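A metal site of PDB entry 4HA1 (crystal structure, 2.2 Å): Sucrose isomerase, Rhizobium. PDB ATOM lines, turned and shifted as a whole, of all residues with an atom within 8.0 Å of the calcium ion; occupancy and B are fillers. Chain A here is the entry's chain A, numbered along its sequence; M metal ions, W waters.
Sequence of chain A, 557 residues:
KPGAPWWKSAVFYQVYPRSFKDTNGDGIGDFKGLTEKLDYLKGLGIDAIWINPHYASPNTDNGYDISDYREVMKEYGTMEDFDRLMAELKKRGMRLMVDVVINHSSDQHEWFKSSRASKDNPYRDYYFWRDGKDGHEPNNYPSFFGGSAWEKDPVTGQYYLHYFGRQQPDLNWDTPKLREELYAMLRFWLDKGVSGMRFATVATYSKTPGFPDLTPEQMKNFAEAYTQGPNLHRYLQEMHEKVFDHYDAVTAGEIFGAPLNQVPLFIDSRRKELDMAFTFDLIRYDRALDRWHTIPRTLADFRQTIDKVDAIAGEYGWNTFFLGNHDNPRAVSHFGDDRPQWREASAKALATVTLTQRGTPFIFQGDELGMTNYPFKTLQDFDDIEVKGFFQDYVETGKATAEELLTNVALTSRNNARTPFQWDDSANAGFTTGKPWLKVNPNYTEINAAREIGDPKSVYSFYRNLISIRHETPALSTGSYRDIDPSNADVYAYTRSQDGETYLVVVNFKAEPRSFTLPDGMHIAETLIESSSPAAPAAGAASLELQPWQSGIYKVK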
ATOM      1  N   PRO A  17       4.211  36.007  11.941  1.00  0.00           N
ATOM      2  CA  PRO A  17       3.705  34.625  11.971  1.00  0.00           C
ATOM      3  C   PRO A  17       4.338  33.738  10.902  1.00  0.00           C
ATOM      4  O   PRO A  17       4.614  32.567  11.152  1.00  0.00           O
ATOM      5  CB  PRO A  17       2.203  34.788  11.728  1.00  0.00           C
ATOM      6  CG  PRO A  17       1.900  36.175  12.165  1.00  0.00           C
ATOM      7  CD  PRO A  17       3.117  36.982  11.815  1.00  0.00           C
ATOM      8  N   ARG A  18       4.573  34.311   9.728  1.00  0.00           N
ATOM      9  CA  ARG A  18       5.205  33.602   8.625  1.00  0.00           C
ATOM     10  C   ARG A  18       6.539  32.955   9.018  1.00  0.00           C
ATOM     11  O   ARG A  18       6.896  31.889   8.516  1.00  0.00           O
ATOM     12  CB  ARG A  18       5.401  34.570   7.452  1.00  0.00           C
ATOM     13  CG  ARG A  18       5.803  33.918   6.155  1.00  0.00           C
ATOM     14  CD  ARG A  18       5.947  34.950   5.051  1.00  0.00           C
ATOM     15  NE  ARG A  18       6.362  34.343   3.798  1.00  0.00           N
ATOM     16  CZ  ARG A  18       5.533  33.886   2.866  1.00  0.00           C
ATOM     17  NH1 ARG A  18       4.222  33.979   3.049  1.00  0.00           N
ATOM     18  NH2 ARG A  18       6.004  33.341   1.757  1.00  0.00           N
ATOM     19  N   LYS A  21       6.539  29.914  13.772  1.00  0.00           N
ATOM     20  CA  LYS A  21       6.465  28.472  14.018  1.00  0.00           C
ATOM     21  C   LYS A  21       5.560  27.756  13.017  1.00  0.00           C
ATOM     22  O   LYS A  21       4.361  28.021  12.937  1.00  0.00           O
ATOM     23  CB  LYS A  21       5.989  28.202  15.446  1.00  0.00           C
ATOM     24  CG  LYS A  21       6.150  26.753  15.880  1.00  0.00           C
ATOM     25  CD  LYS A  21       7.595  26.285  15.764  1.00  0.00           C
ATOM     26  CE  LYS A  21       7.767  24.873  16.291  1.00  0.00           C
ATOM     27  NZ  LYS A  21       6.968  23.870  15.532  1.00  0.00           N
ATOM     28  N   ASP A  22       6.174  26.830  12.265  1.00  0.00           N
ATOM     29  CA  ASP A  22       5.442  26.000  11.320  1.00  0.00           C
ATOM     30  C   ASP A  22       5.029  24.693  11.999  1.00  0.00           C
ATOM     31  O   ASP A  22       5.762  24.169  12.834  1.00  0.00           O
ATOM     32  CB  ASP A  22       6.330  25.715  10.097  1.00  0.00           C
ATOM     33  CG  ASP A  22       5.636  24.869   9.047  1.00  0.00           C
ATOM     34  OD1 ASP A  22       4.394  24.793   9.055  1.00  0.00           O
ATOM     35  OD2 ASP A  22       6.344  24.268   8.203  1.00  0.00           O
ATOM     36  N   THR A  23       3.857  24.185  11.652  1.00  0.00           N
ATOM     37  CA  THR A  23       3.371  22.926  12.243  1.00  0.00           C
ATOM     38  C   THR A  23       2.869  21.904  11.229  1.00  0.00           C
ATOM     39  O   THR A  23       2.420  20.828  11.603  1.00  0.00           O
ATOM     40  CB  THR A  23       2.245  23.168  13.271  1.00  0.00           C
ATOM     41  OG1 THR A  23       1.215  23.960  12.686  1.00  0.00           O
ATOM     42  CG2 THR A  23       2.779  23.858  14.518  1.00  0.00           C
ATOM     43  N   ASN A  24       2.936  22.236   9.939  1.00  0.00           N
ATOM     44  CA  ASN A  24       2.473  21.305   8.913  1.00  0.00           C
ATOM     45  C   ASN A  24       3.503  21.058   7.803  1.00  0.00           C
ATOM     46  O   ASN A  24       3.160  20.555   6.743  1.00  0.00           O
ATOM     47  CB  ASN A  24       1.134  21.745   8.326  1.00  0.00           C
ATOM     48  CG  ASN A  24       1.251  22.981   7.470  1.00  0.00           C
ATOM     49  OD1 ASN A  24       2.208  23.755   7.604  1.00  0.00           O
ATOM     50  ND2 ASN A  24       0.287  23.191   6.580  1.00  0.00           N
ATOM     51  N   GLY A  25       4.745  21.433   8.081  1.00  0.00           N
ATOM     52  CA  GLY A  25       5.849  21.159   7.179  1.00  0.00           C
ATOM     53  C   GLY A  25       5.766  21.765   5.793  1.00  0.00           C
ATOM     54  O   GLY A  25       6.256  21.180   4.826  1.00  0.00           O
ATOM     55  N   ASP A  26       5.160  22.944   5.691  1.00  0.00           N
ATOM     56  CA  ASP A  26       5.092  23.637   4.405  1.00  0.00           C
ATOM     57  C   ASP A  26       6.174  24.706   4.313  1.00  0.00           C
ATOM     58  O   ASP A  26       6.344  25.342   3.278  1.00  0.00           O
ATOM     59  CB  ASP A  26       3.705  24.249   4.178  1.00  0.00           C
ATOM     60  CG  ASP A  26       3.381  25.361   5.164  1.00  0.00           C
ATOM     61  OD1 ASP A  26       4.085  25.488   6.187  1.00  0.00           O
ATOM     62  OD2 ASP A  26       2.411  26.110   4.914  1.00  0.00           O
ATOM     63  N   GLY A  27       6.898  24.892   5.409  1.00  0.00           N
ATOM     64  CA  GLY A  27       7.976  25.860   5.457  1.00  0.00           C
ATOM     65  C   GLY A  27       7.493  27.246   5.851  1.00  0.00           C
ATOM     66  O   GLY A  27       8.262  28.210   5.836  1.00  0.00           O
ATOM     67  N   ILE A  28       6.215  27.342   6.191  1.00  0.00           N
ATOM     68  CA  ILE A  28       5.626  28.622   6.557  1.00  0.00           C
ATOM     69  C   ILE A  28       5.033  28.573   7.960  1.00  0.00           C
ATOM     70  O   ILE A  28       4.319  27.621   8.296  1.00  0.00           O
ATOM     71  CB  ILE A  28       4.530  29.044   5.549  1.00  0.00           C
ATOM     72  CG1 ILE A  28       5.131  29.179   4.147  1.00  0.00           C
ATOM     73  CG2 ILE A  28       3.863  30.349   5.990  1.00  0.00           C
ATOM     74  CD1 ILE A  28       4.125  29.556   3.072  1.00  0.00           C
ATOM     75  N   GLY A  29       5.336  29.571   8.782  1.00  0.00           N
ATOM     76  CA  GLY A  29       4.770  29.661  10.109  1.00  0.00           C
ATOM     77  C   GLY A  29       3.269  29.838  10.037  1.00  0.00           C
ATOM     78  O   GLY A  29       2.753  30.367   9.048  1.00  0.00           O
ATOM     79  N   ASP A  30       2.561  29.391  11.063  1.00  0.00           N
ATOM     80  CA  ASP A  30       1.103  29.437  11.055  1.00  0.00           C
ATOM     81  C   ASP A  30       0.542  29.706  12.448  1.00  0.00           C
ATOM     82  O   ASP A  30       1.292  29.811  13.417  1.00  0.00           O
ATOM     83  CB  ASP A  30       0.545  28.122  10.503  1.00  0.00           C
ATOM     84  CG  ASP A  30       1.214  26.907  11.103  1.00  0.00           C
ATOM     85  OD1 ASP A  30       0.909  26.574  12.269  1.00  0.00           O
ATOM     86  OD2 ASP A  30       2.039  26.285  10.413  1.00  0.00           O
ATOM     87  N   PHE A  31      -0.787  29.818  12.539  1.00  0.00           N
ATOM     88  CA  PHE A  31      -1.455  30.110  13.792  1.00  0.00           C
ATOM     89  C   PHE A  31      -1.274  29.004  14.825  1.00  0.00           C
ATOM     90  O   PHE A  31      -1.028  29.274  15.999  1.00  0.00           O
ATOM     91  CB  PHE A  31      -2.949  30.359  13.565  1.00  0.00           C
ATOM     92  CG  PHE A  31      -3.257  31.733  13.053  1.00  0.00           C
ATOM     93  CD1 PHE A  31      -2.460  32.815  13.409  1.00  0.00           C
ATOM     94  CD2 PHE A  31      -4.335  31.943  12.214  1.00  0.00           C
ATOM     95  CE1 PHE A  31      -2.747  34.077  12.939  1.00  0.00           C
ATOM     96  CE2 PHE A  31      -4.612  33.214  11.738  1.00  0.00           C
ATOM     97  CZ  PHE A  31      -3.823  34.280  12.107  1.00  0.00           C
ATOM     98  N   LYS A  32      -1.411  27.755  14.377  1.00  0.00           N
ATOM     99  CA  LYS A  32      -1.240  26.620  15.267  1.00  0.00           C
ATOM    100  C   LYS A  32       0.155  26.613  15.888  1.00  0.00           C
ATOM    101  O   LYS A  32       0.339  26.177  17.026  1.00  0.00           O
ATOM    102  CB  LYS A  32      -1.496  25.300  14.516  1.00  0.00           C
ATOM    103  N   GLY A  33       1.134  27.122  15.143  1.00  0.00           N
ATOM    104  CA  GLY A  33       2.477  27.245  15.657  1.00  0.00           C
ATOM    105  C   GLY A  33       2.590  28.289  16.754  1.00  0.00           C
ATOM    106  O   GLY A  33       3.228  28.060  17.778  1.00  0.00           O
ATOM    107  N   LYS A  74      -4.842  31.915   4.150  1.00  0.00           N
ATOM    108  CA  LYS A  74      -4.866  30.459   3.996  1.00  0.00           C
ATOM    109  C   LYS A  74      -3.607  29.788   4.542  1.00  0.00           C
ATOM    110  O   LYS A  74      -3.678  28.694   5.110  1.00  0.00           O
ATOM    111  CB  LYS A  74      -5.055  30.090   2.519  1.00  0.00           C
ATOM    112  N   GLU A  75      -2.459  30.437   4.379  1.00  0.00           N
ATOM    113  CA  GLU A  75      -1.206  29.900   4.890  1.00  0.00           C
ATOM    114  C   GLU A  75      -1.208  29.768   6.418  1.00  0.00           C
ATOM    115  O   GLU A  75      -0.614  28.843   6.961  1.00  0.00           O
ATOM    116  CB  GLU A  75      -0.021  30.761   4.440  1.00  0.00           C
ATOM    117  CG  GLU A  75       0.462  30.483   3.016  1.00  0.00           C
ATOM    118  CD  GLU A  75      -0.328  31.221   1.960  1.00  0.00           C
ATOM    119  OE1 GLU A  75      -1.194  32.046   2.332  1.00  0.00           O
ATOM    120  OE2 GLU A  75      -0.074  30.999   0.752  1.00  0.00           O
ATOM    121  N   TYR A  76      -1.889  30.693   7.103  1.00  0.00           N
ATOM    122  CA  TYR A  76      -1.858  30.714   8.570  1.00  0.00           C
ATOM    123  C   TYR A  76      -2.901  29.785   9.210  1.00  0.00           C
ATOM    124  O   TYR A  76      -2.788  29.418  10.380  1.00  0.00           O
ATOM    125  CB  TYR A  76      -1.988  32.136   9.114  1.00  0.00           C
ATOM    126  CG  TYR A  76      -0.874  33.074   8.675  1.00  0.00           C
ATOM    127  CD1 TYR A  76       0.283  32.585   8.079  1.00  0.00           C
ATOM    128  CD2 TYR A  76      -0.983  34.449   8.859  1.00  0.00           C
ATOM    129  CE1 TYR A  76       1.294  33.439   7.678  1.00  0.00           C
ATOM    130  CE2 TYR A  76       0.018  35.309   8.464  1.00  0.00           C
ATOM    131  CZ  TYR A  76       1.157  34.796   7.874  1.00  0.00           C
ATOM    132  OH  TYR A  76       2.170  35.643   7.465  1.00  0.00           O
ATOM    133  N   GLY A  77      -3.919  29.411   8.432  1.00  0.00           N
ATOM    134  CA  GLY A  77      -4.962  28.532   8.938  1.00  0.00           C
ATOM    135  C   GLY A  77      -6.356  29.008   8.575  1.00  0.00           C
ATOM    136  O   GLY A  77      -6.571  29.582   7.509  1.00  0.00           O
ATOM    137  N   PHE A 431      12.144  25.146  13.565  1.00  0.00           N
ATOM    138  CA  PHE A 431      11.079  25.970  13.000  1.00  0.00           C
ATOM    139  C   PHE A 431      10.122  25.134  12.151  1.00  0.00           C
ATOM    140  O   PHE A 431       8.898  25.280  12.253  1.00  0.00           O
ATOM    141  CB  PHE A 431      11.669  27.121  12.179  1.00  0.00           C
ATOM    142  CG  PHE A 431      10.664  27.818  11.312  1.00  0.00           C
ATOM    143  CD1 PHE A 431       9.707  28.660  11.864  1.00  0.00           C
ATOM    144  CD2 PHE A 431      10.677  27.645   9.931  1.00  0.00           C
ATOM    145  CE1 PHE A 431       8.786  29.303  11.064  1.00  0.00           C
ATOM    146  CE2 PHE A 431       9.756  28.288   9.131  1.00  0.00           C
ATOM    147  CZ  PHE A 431       8.810  29.124   9.690  1.00  0.00           C
ATOM    148  N   THR A 432      10.682  24.258  11.326  1.00  0.00           N
ATOM    149  CA  THR A 432       9.875  23.454  10.413  1.00  0.00           C
ATOM    150  C   THR A 432      10.481  22.084  10.153  1.00  0.00           C
ATOM    151  O   THR A 432      11.699  21.900  10.270  1.00  0.00           O
ATOM    152  CB  THR A 432       9.665  24.173   9.065  1.00  0.00           C
ATOM    153  OG1 THR A 432       8.825  23.372   8.214  1.00  0.00           O
ATOM    154  CG2 THR A 432      10.999  24.411   8.376  1.00  0.00           C
HETATM  155 CA    CA M   1       2.634  26.037   7.989  1.00  0.00          CA
HETATM  156  O   HOH W   1       1.382  27.567   6.487  1.00  0.00           O
HETATM  157  O   HOH W   2       0.160  25.851   7.884  1.00  0.00           O
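The side-chain carboxylate of Asp 22 sits at hydrogen-bond distance from the backbone NH of Gly 25 (3.3 Å). OD2 of Asp 22 sits at hydrogen-bond distance from N of Gly 27 (2.9 Å). The side-chain carboxylate of Asp 22 sits at hydrogen-bond distance from the side-chain hydroxyl of Thr 432, 2.6 Å away. The backbone carbonyl oxygen (O) of Phe 431 lies within hydrogen-bond range of the backbone NH (N) of Asp 22. The side-chain hydroxyl (OG1) of Thr 23 is in hydrogen-bond range of the side-chain carboxylate (OD1) of Asp 30, at 2.7 Å. N of Asp 30 sits at hydrogen-bond distance from O of Lys 21, 2.9 Å away. The side-chain carboxylate of Asp 30 lies within hydrogen-bond range of the backbone NH of Gly 33 (2.9 Å). OD1 of Asp 30 lies within hydrogen-bond range of N of Lys 32 (3.3 Å).
Five residues have an atom within 4 Å of the calcium ion: Asp 22, Asn 24, Asp 26, Ile 28 and Asp 30. The nearest printed residue that does not touch the calcium ion is Thr 23 (4.3 Å).
The calcium ion is bound by O of Ile 28, OD1 of Asn 24, OD1 of Asp 26, OD1 of Asp 22, water W1, water W2 and OD2 of Asp 30. Slightly farther from the calcium ion lies OD2 of Asp 26 (3.1 Å).
Water W2 lies within hydrogen-bond range of the side-chain amide nitrogen (ND2) of Asn 24 (3.0 Å) and the backbone carbonyl oxygen (O) of Glu 75 (3.2 Å).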
